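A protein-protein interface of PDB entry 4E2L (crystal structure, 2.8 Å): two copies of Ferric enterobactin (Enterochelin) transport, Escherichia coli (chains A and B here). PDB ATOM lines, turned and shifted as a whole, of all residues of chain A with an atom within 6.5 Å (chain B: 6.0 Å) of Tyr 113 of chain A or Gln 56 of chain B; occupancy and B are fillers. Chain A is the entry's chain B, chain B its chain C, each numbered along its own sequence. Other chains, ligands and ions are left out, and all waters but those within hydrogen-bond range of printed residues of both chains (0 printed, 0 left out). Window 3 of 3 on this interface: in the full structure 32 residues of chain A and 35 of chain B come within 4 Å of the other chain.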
ATOM      1  N   THR A  16       0.975  19.943   1.861  1.00  0.00           N
ATOM      2  CA  THR A  16       2.299  19.567   2.326  1.00  0.00           C
ATOM      3  C   THR A  16       2.254  18.166   2.962  1.00  0.00           C
ATOM      4  O   THR A  16       1.203  17.744   3.421  1.00  0.00           O
ATOM      5  CB  THR A  16       2.786  20.593   3.358  1.00  0.00           C
ATOM      6  OG1 THR A  16       4.169  20.880   3.133  1.00  0.00           O
ATOM      7  CG2 THR A  16       2.585  20.077   4.771  1.00  0.00           C
ATOM      8  N   PRO A  17       3.385  17.431   2.962  1.00  0.00           N
ATOM      9  CA  PRO A  17       3.494  16.151   3.681  1.00  0.00           C
ATOM     10  C   PRO A  17       3.022  16.267   5.125  1.00  0.00           C
ATOM     11  O   PRO A  17       3.383  17.216   5.804  1.00  0.00           O
ATOM     12  CB  PRO A  17       4.992  15.859   3.631  1.00  0.00           C
ATOM     13  CG  PRO A  17       5.395  16.417   2.323  1.00  0.00           C
ATOM     14  CD  PRO A  17       4.570  17.670   2.122  1.00  0.00           C
ATOM     15  N   SER A 111      15.114  24.209   0.008  1.00  0.00           N
ATOM     16  CA  SER A 111      13.682  24.399   0.233  1.00  0.00           C
ATOM     17  C   SER A 111      13.277  23.843   1.586  1.00  0.00           C
ATOM     18  O   SER A 111      13.451  22.654   1.846  1.00  0.00           O
ATOM     19  CB  SER A 111      12.867  23.701  -0.853  1.00  0.00           C
ATOM     20  OG  SER A 111      11.545  24.213  -0.891  1.00  0.00           O
ATOM     21  N   LEU A 112      12.721  24.698   2.439  1.00  0.00           N
ATOM     22  CA  LEU A 112      12.413  24.302   3.808  1.00  0.00           C
ATOM     23  C   LEU A 112      11.633  22.994   3.848  1.00  0.00           C
ATOM     24  O   LEU A 112      12.174  21.968   4.251  1.00  0.00           O
ATOM     25  CB  LEU A 112      11.674  25.411   4.554  1.00  0.00           C
ATOM     26  CG  LEU A 112      11.622  25.299   6.083  1.00  0.00           C
ATOM     27  CD1 LEU A 112      13.014  25.087   6.687  1.00  0.00           C
ATOM     28  CD2 LEU A 112      10.957  26.530   6.691  1.00  0.00           C
ATOM     29  N   TYR A 113      10.372  23.029   3.418  1.00  0.00           N
ATOM     30  CA  TYR A 113       9.530  21.825   3.358  1.00  0.00           C
ATOM     31  C   TYR A 113       9.060  21.585   1.927  1.00  0.00           C
ATOM     32  O   TYR A 113       9.230  22.446   1.073  1.00  0.00           O
ATOM     33  CB  TYR A 113       8.326  21.973   4.282  1.00  0.00           C
ATOM     34  CG  TYR A 113       7.609  23.269   4.078  1.00  0.00           C
ATOM     35  CD1 TYR A 113       6.652  23.400   3.077  1.00  0.00           C
ATOM     36  CD2 TYR A 113       7.909  24.384   4.856  1.00  0.00           C
ATOM     37  CE1 TYR A 113       5.989  24.600   2.873  1.00  0.00           C
ATOM     38  CE2 TYR A 113       7.257  25.594   4.659  1.00  0.00           C
ATOM     39  CZ  TYR A 113       6.297  25.693   3.667  1.00  0.00           C
ATOM     40  OH  TYR A 113       5.640  26.889   3.464  1.00  0.00           O
ATOM     41  N   THR A 114       8.488  20.413   1.663  1.00  0.00           N
ATOM     42  CA  THR A 114       7.970  20.102   0.337  1.00  0.00           C
ATOM     43  C   THR A 114       6.517  20.513   0.246  1.00  0.00           C
ATOM     44  O   THR A 114       5.763  20.274   1.184  1.00  0.00           O
ATOM     45  CB  THR A 114       8.067  18.613   0.029  1.00  0.00           C
ATOM     46  OG1 THR A 114       9.419  18.301  -0.319  1.00  0.00           O
ATOM     47  CG2 THR A 114       7.144  18.243  -1.138  1.00  0.00           C
ATOM     48  N   SER A 115       6.124  21.137  -0.868  1.00  0.00           N
ATOM     49  CA  SER A 115       4.732  21.556  -1.037  1.00  0.00           C
ATOM     50  C   SER A 115       4.281  21.631  -2.497  1.00  0.00           C
ATOM     51  O   SER A 115       5.029  22.069  -3.380  1.00  0.00           O
ATOM     52  CB  SER A 115       4.471  22.886  -0.329  1.00  0.00           C
ATOM     53  OG  SER A 115       4.992  23.985  -1.056  1.00  0.00           O
ATOM     54  N   GLN A 264      -1.575  23.827   3.754  1.00  0.00           N
ATOM     55  CA  GLN A 264      -1.124  25.204   3.938  1.00  0.00           C
ATOM     56  C   GLN A 264      -2.318  26.074   3.558  1.00  0.00           C
ATOM     57  O   GLN A 264      -2.735  26.953   4.314  1.00  0.00           O
ATOM     58  CB  GLN A 264       0.072  25.532   3.043  1.00  0.00           C
ATOM     59  CG  GLN A 264       1.444  25.028   3.528  1.00  0.00           C
ATOM     60  CD  GLN A 264       1.777  25.444   4.949  1.00  0.00           C
ATOM     61  OE1 GLN A 264       1.446  24.737   5.903  1.00  0.00           O
ATOM     62  NE2 GLN A 264       2.450  26.577   5.098  1.00  0.00           N
ATOM     63  N   ASN B  49      11.590  25.885  12.448  1.00  0.00           N
ATOM     64  CA  ASN B  49      11.167  25.556  11.101  1.00  0.00           C
ATOM     65  C   ASN B  49       9.670  25.279  11.027  1.00  0.00           C
ATOM     66  O   ASN B  49       9.060  25.399   9.957  1.00  0.00           O
ATOM     67  CB  ASN B  49      11.950  24.357  10.570  1.00  0.00           C
ATOM     68  CG  ASN B  49      13.414  24.682  10.302  1.00  0.00           C
ATOM     69  OD1 ASN B  49      13.845  25.842  10.381  1.00  0.00           O
ATOM     70  ND2 ASN B  49      14.188  23.651   9.970  1.00  0.00           N
ATOM     71  N   PHE B  51       7.570  26.882  13.231  1.00  0.00           N
ATOM     72  CA  PHE B  51       7.046  28.239  13.360  1.00  0.00           C
ATOM     73  C   PHE B  51       6.966  28.931  12.019  1.00  0.00           C
ATOM     74  O   PHE B  51       5.981  29.576  11.731  1.00  0.00           O
ATOM     75  CB  PHE B  51       7.919  29.087  14.257  1.00  0.00           C
ATOM     76  CG  PHE B  51       7.466  30.504  14.360  1.00  0.00           C
ATOM     77  CD1 PHE B  51       6.389  30.841  15.160  1.00  0.00           C
ATOM     78  CD2 PHE B  51       8.116  31.499  13.662  1.00  0.00           C
ATOM     79  CE1 PHE B  51       5.968  32.141  15.271  1.00  0.00           C
ATOM     80  CE2 PHE B  51       7.703  32.803  13.765  1.00  0.00           C
ATOM     81  CZ  PHE B  51       6.627  33.130  14.574  1.00  0.00           C
ATOM     82  N   ILE B  52       8.014  28.808  11.214  1.00  0.00           N
ATOM     83  CA  ILE B  52       8.068  29.479   9.924  1.00  0.00           C
ATOM     84  C   ILE B  52       7.104  28.868   8.908  1.00  0.00           C
ATOM     85  O   ILE B  52       6.502  29.589   8.096  1.00  0.00           O
ATOM     86  CB  ILE B  52       9.512  29.558   9.359  1.00  0.00           C
ATOM     87  CG1 ILE B  52      10.341  30.583  10.144  1.00  0.00           C
ATOM     88  CG2 ILE B  52       9.505  29.931   7.884  1.00  0.00           C
ATOM     89  CD1 ILE B  52       9.802  32.001  10.093  1.00  0.00           C
ATOM     90  N   LYS B  53       6.941  27.550   8.967  1.00  0.00           N
ATOM     91  CA  LYS B  53       5.983  26.868   8.106  1.00  0.00           C
ATOM     92  C   LYS B  53       4.541  27.241   8.455  1.00  0.00           C
ATOM     93  O   LYS B  53       3.741  27.579   7.576  1.00  0.00           O
ATOM     94  CB  LYS B  53       6.171  25.359   8.194  1.00  0.00           C
ATOM     95  CG  LYS B  53       5.110  24.571   7.482  1.00  0.00           C
ATOM     96  CD  LYS B  53       5.683  23.381   6.745  1.00  0.00           C
ATOM     97  CE  LYS B  53       4.600  22.347   6.506  1.00  0.00           C
ATOM     98  NZ  LYS B  53       4.078  21.845   7.817  1.00  0.00           N
ATOM     99  N   LYS B  54       4.195  27.183   9.732  1.00  0.00           N
ATOM    100  CA  LYS B  54       2.857  27.601  10.125  1.00  0.00           C
ATOM    101  C   LYS B  54       2.545  29.074   9.811  1.00  0.00           C
ATOM    102  O   LYS B  54       1.408  29.428   9.538  1.00  0.00           O
ATOM    103  CB  LYS B  54       2.607  27.277  11.595  1.00  0.00           C
ATOM    104  CG  LYS B  54       2.150  25.860  11.817  1.00  0.00           C
ATOM    105  CD  LYS B  54       1.747  25.623  13.257  1.00  0.00           C
ATOM    106  CE  LYS B  54       1.612  24.140  13.524  1.00  0.00           C
ATOM    107  NZ  LYS B  54       0.971  23.445  12.364  1.00  0.00           N
ATOM    108  N   PHE B  55       3.566  29.922   9.848  1.00  0.00           N
ATOM    109  CA  PHE B  55       3.419  31.356   9.600  1.00  0.00           C
ATOM    110  C   PHE B  55       3.207  31.638   8.122  1.00  0.00           C
ATOM    111  O   PHE B  55       2.481  32.546   7.783  1.00  0.00           O
ATOM    112  CB  PHE B  55       4.663  32.091  10.090  1.00  0.00           C
ATOM    113  CG  PHE B  55       4.653  33.580   9.854  1.00  0.00           C
ATOM    114  CD1 PHE B  55       4.449  34.460  10.907  1.00  0.00           C
ATOM    115  CD2 PHE B  55       4.913  34.105   8.595  1.00  0.00           C
ATOM    116  CE1 PHE B  55       4.475  35.824  10.693  1.00  0.00           C
ATOM    117  CE2 PHE B  55       4.939  35.462   8.388  1.00  0.00           C
ATOM    118  CZ  PHE B  55       4.718  36.317   9.431  1.00  0.00           C
ATOM    119  N   GLN B  56       3.845  30.861   7.254  1.00  0.00           N
ATOM    120  CA  GLN B  56       3.625  30.944   5.817  1.00  0.00           C
ATOM    121  C   GLN B  56       2.266  30.357   5.366  1.00  0.00           C
ATOM    122  O   GLN B  56       1.963  30.294   4.165  1.00  0.00           O
ATOM    123  CB  GLN B  56       4.770  30.251   5.076  1.00  0.00           C
ATOM    124  CG  GLN B  56       6.062  31.052   4.996  1.00  0.00           C
ATOM    125  CD  GLN B  56       7.198  30.248   4.390  1.00  0.00           C
ATOM    126  OE1 GLN B  56       7.216  29.021   4.465  1.00  0.00           O
ATOM    127  NE2 GLN B  56       8.150  30.931   3.784  1.00  0.00           N
ATOM    128  N   SER B  57       1.442  29.936   6.321  1.00  0.00           N
ATOM    129  CA  SER B  57       0.158  29.326   5.974  1.00  0.00           C
ATOM    130  C   SER B  57      -0.937  30.354   5.707  1.00  0.00           C
ATOM    131  O   SER B  57      -1.406  31.003   6.642  1.00  0.00           O
ATOM    132  CB  SER B  57      -0.307  28.370   7.074  1.00  0.00           C
ATOM    133  OG  SER B  57      -1.648  27.960   6.849  1.00  0.00           O
ATOM    134  N   VAL B  58      -1.367  30.484   4.449  1.00  0.00           N
ATOM    135  CA  VAL B  58      -2.406  31.470   4.127  1.00  0.00           C
ATOM    136  C   VAL B  58      -3.707  31.164   4.874  1.00  0.00           C
ATOM    137  O   VAL B  58      -4.349  32.063   5.422  1.00  0.00           O
ATOM    138  CB  VAL B  58      -2.691  31.598   2.590  1.00  0.00           C
ATOM    139  CG1 VAL B  58      -4.003  32.327   2.331  1.00  0.00           C
ATOM    140  CG2 VAL B  58      -1.551  32.302   1.862  1.00  0.00           C
ATOM    141  N   ALA B  98       7.011  36.767   4.934  1.00  0.00           N
ATOM    142  CA  ALA B  98       8.129  36.151   5.640  1.00  0.00           C
ATOM    143  C   ALA B  98       9.308  35.944   4.693  1.00  0.00           C
ATOM    144  O   ALA B  98       9.175  35.305   3.645  1.00  0.00           O
ATOM    145  CB  ALA B  98       7.703  34.811   6.287  1.00  0.00           C
ATOM    146  N   TRP B 116      15.119  34.925   9.863  1.00  0.00           N
ATOM    147  CA  TRP B 116      14.045  35.270   8.937  1.00  0.00           C
ATOM    148  C   TRP B 116      13.479  36.629   9.312  1.00  0.00           C
ATOM    149  O   TRP B 116      13.372  36.951  10.496  1.00  0.00           O
ATOM    150  CB  TRP B 116      12.933  34.221   8.969  1.00  0.00           C
ATOM    151  CG  TRP B 116      13.242  32.943   8.227  1.00  0.00           C
ATOM    152  CD1 TRP B 116      14.226  32.049   8.511  1.00  0.00           C
ATOM    153  CD2 TRP B 116      12.532  32.409   7.100  1.00  0.00           C
ATOM    154  NE1 TRP B 116      14.193  30.999   7.625  1.00  0.00           N
ATOM    155  CE2 TRP B 116      13.160  31.193   6.749  1.00  0.00           C
ATOM    156  CE3 TRP B 116      11.436  32.847   6.345  1.00  0.00           C
ATOM    157  CZ2 TRP B 116      12.724  30.407   5.681  1.00  0.00           C
ATOM    158  CZ3 TRP B 116      11.006  32.065   5.286  1.00  0.00           C
ATOM    159  CH2 TRP B 116      11.649  30.858   4.965  1.00  0.00           C
ATOM    160  N   TYR B 135      -0.293  38.295  15.370  1.00  0.00           N
ATOM    161  CA  TYR B 135      -0.230  37.114  14.519  1.00  0.00           C
ATOM    162  C   TYR B 135       0.953  36.222  14.857  1.00  0.00           C
ATOM    163  O   TYR B 135       0.909  35.016  14.642  1.00  0.00           O
ATOM    164  CB  TYR B 135      -0.122  37.515  13.060  1.00  0.00           C
ATOM    165  CG  TYR B 135      -0.063  36.338  12.123  1.00  0.00           C
ATOM    166  CD1 TYR B 135      -1.038  35.350  12.169  1.00  0.00           C
ATOM    167  CD2 TYR B 135       0.953  36.213  11.186  1.00  0.00           C
ATOM    168  CE1 TYR B 135      -1.000  34.266  11.308  1.00  0.00           C
ATOM    169  CE2 TYR B 135       0.997  35.139  10.315  1.00  0.00           C
ATOM    170  CZ  TYR B 135       0.019  34.166  10.379  1.00  0.00           C
ATOM    171  OH  TYR B 135       0.051  33.081   9.527  1.00  0.00           O
ATOM    172  N   ILE B 139       0.547  32.208  15.951  1.00  0.00           N
ATOM    173  CA  ILE B 139       1.214  31.042  15.377  1.00  0.00           C
ATOM    174  C   ILE B 139       2.093  30.361  16.420  1.00  0.00           C
ATOM    175  O   ILE B 139       2.184  29.134  16.479  1.00  0.00           O
ATOM    176  CB  ILE B 139       2.072  31.403  14.148  1.00  0.00           C
ATOM    177  CG1 ILE B 139       1.192  31.881  12.979  1.00  0.00           C
ATOM    178  CG2 ILE B 139       2.913  30.208  13.720  1.00  0.00           C
ATOM    179  CD1 ILE B 139       0.621  30.765  12.121  1.00  0.00           C
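The side-chain hydroxyl (OH) of Tyr 113 of chain A is in hydrogen-bond range of the side-chain amide oxygen (OE1) of Gln 56 of chain B, 2.8 Å away. O of Gln 264 of chain A is in hydrogen-bond range of OG of Ser 57 of chain B (2.9 Å). The backbone carbonyl oxygen (O) of Lys 53 of chain B is in hydrogen-bond range of the side-chain amide nitrogen (NE2) of Gln 264 of chain A (3.0 Å).
The side-chain hydroxyl of Thr 16 of chain A is in hydrogen-bond range of the backbone carbonyl oxygen of Thr 114 of chain A, 2.6 Å away.
Thr 16 of chain A touches Lys 53 of chain B (CG2 to CE, 3.5 Å). Leu 112 of chain A touches Asn 49 of chain B. Ile 52 of chain B touches Leu 112 of chain A (CG2 to CD2, 3.9 Å). CD of Lys 53 of chain B touches CD2 of Tyr 113 of chain A, 3.1 Å away. Gln 264 of chain A touches Gln 56 of chain B (NE2 to C, 3.8 Å). Gln 264 of chain A touches Val 58 of chain B (O to N, 3.8 Å).
Of the printed residues of chain B, Thr 16 of chain A touches Lys 53 (3.5 Å). Of the printed residues of chain B, Leu 112 of chain A touches Asn 49 and Ile 52. Of the printed residues of chain B, Gln 264 of chain A touches Lys 53 (3.0 Å), Gln 56 (3.8 Å), Ser 57 (2.9 Å) and Val 58 (3.8 Å). Printed residues of chain A within 4 Å of Asn 49 of chain B: Leu 112. Gln 56 of chain B touches just these residues of chain A: Tyr 113 and Gln 264. Printed residues of chain A within 4 Å of Val 58 of chain B: Gln 264. Tyr 135 of chain B touches none of the printed residues of chain A. Ile 139 of chain B touches none of the printed residues of chain A. The nearest printed residue of chain B that does not touch Tyr 113 of chain A is Ile 52 of chain B (5.3 Å).
Of the 8 printed residues of chain A, 4 touch a printed residue of chain B. Among the printed residues, no Asp or Glu carboxylate lies within 4 Å of a Lys or Arg side-chain nitrogen of the other chain.
No position is printed for both chains.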
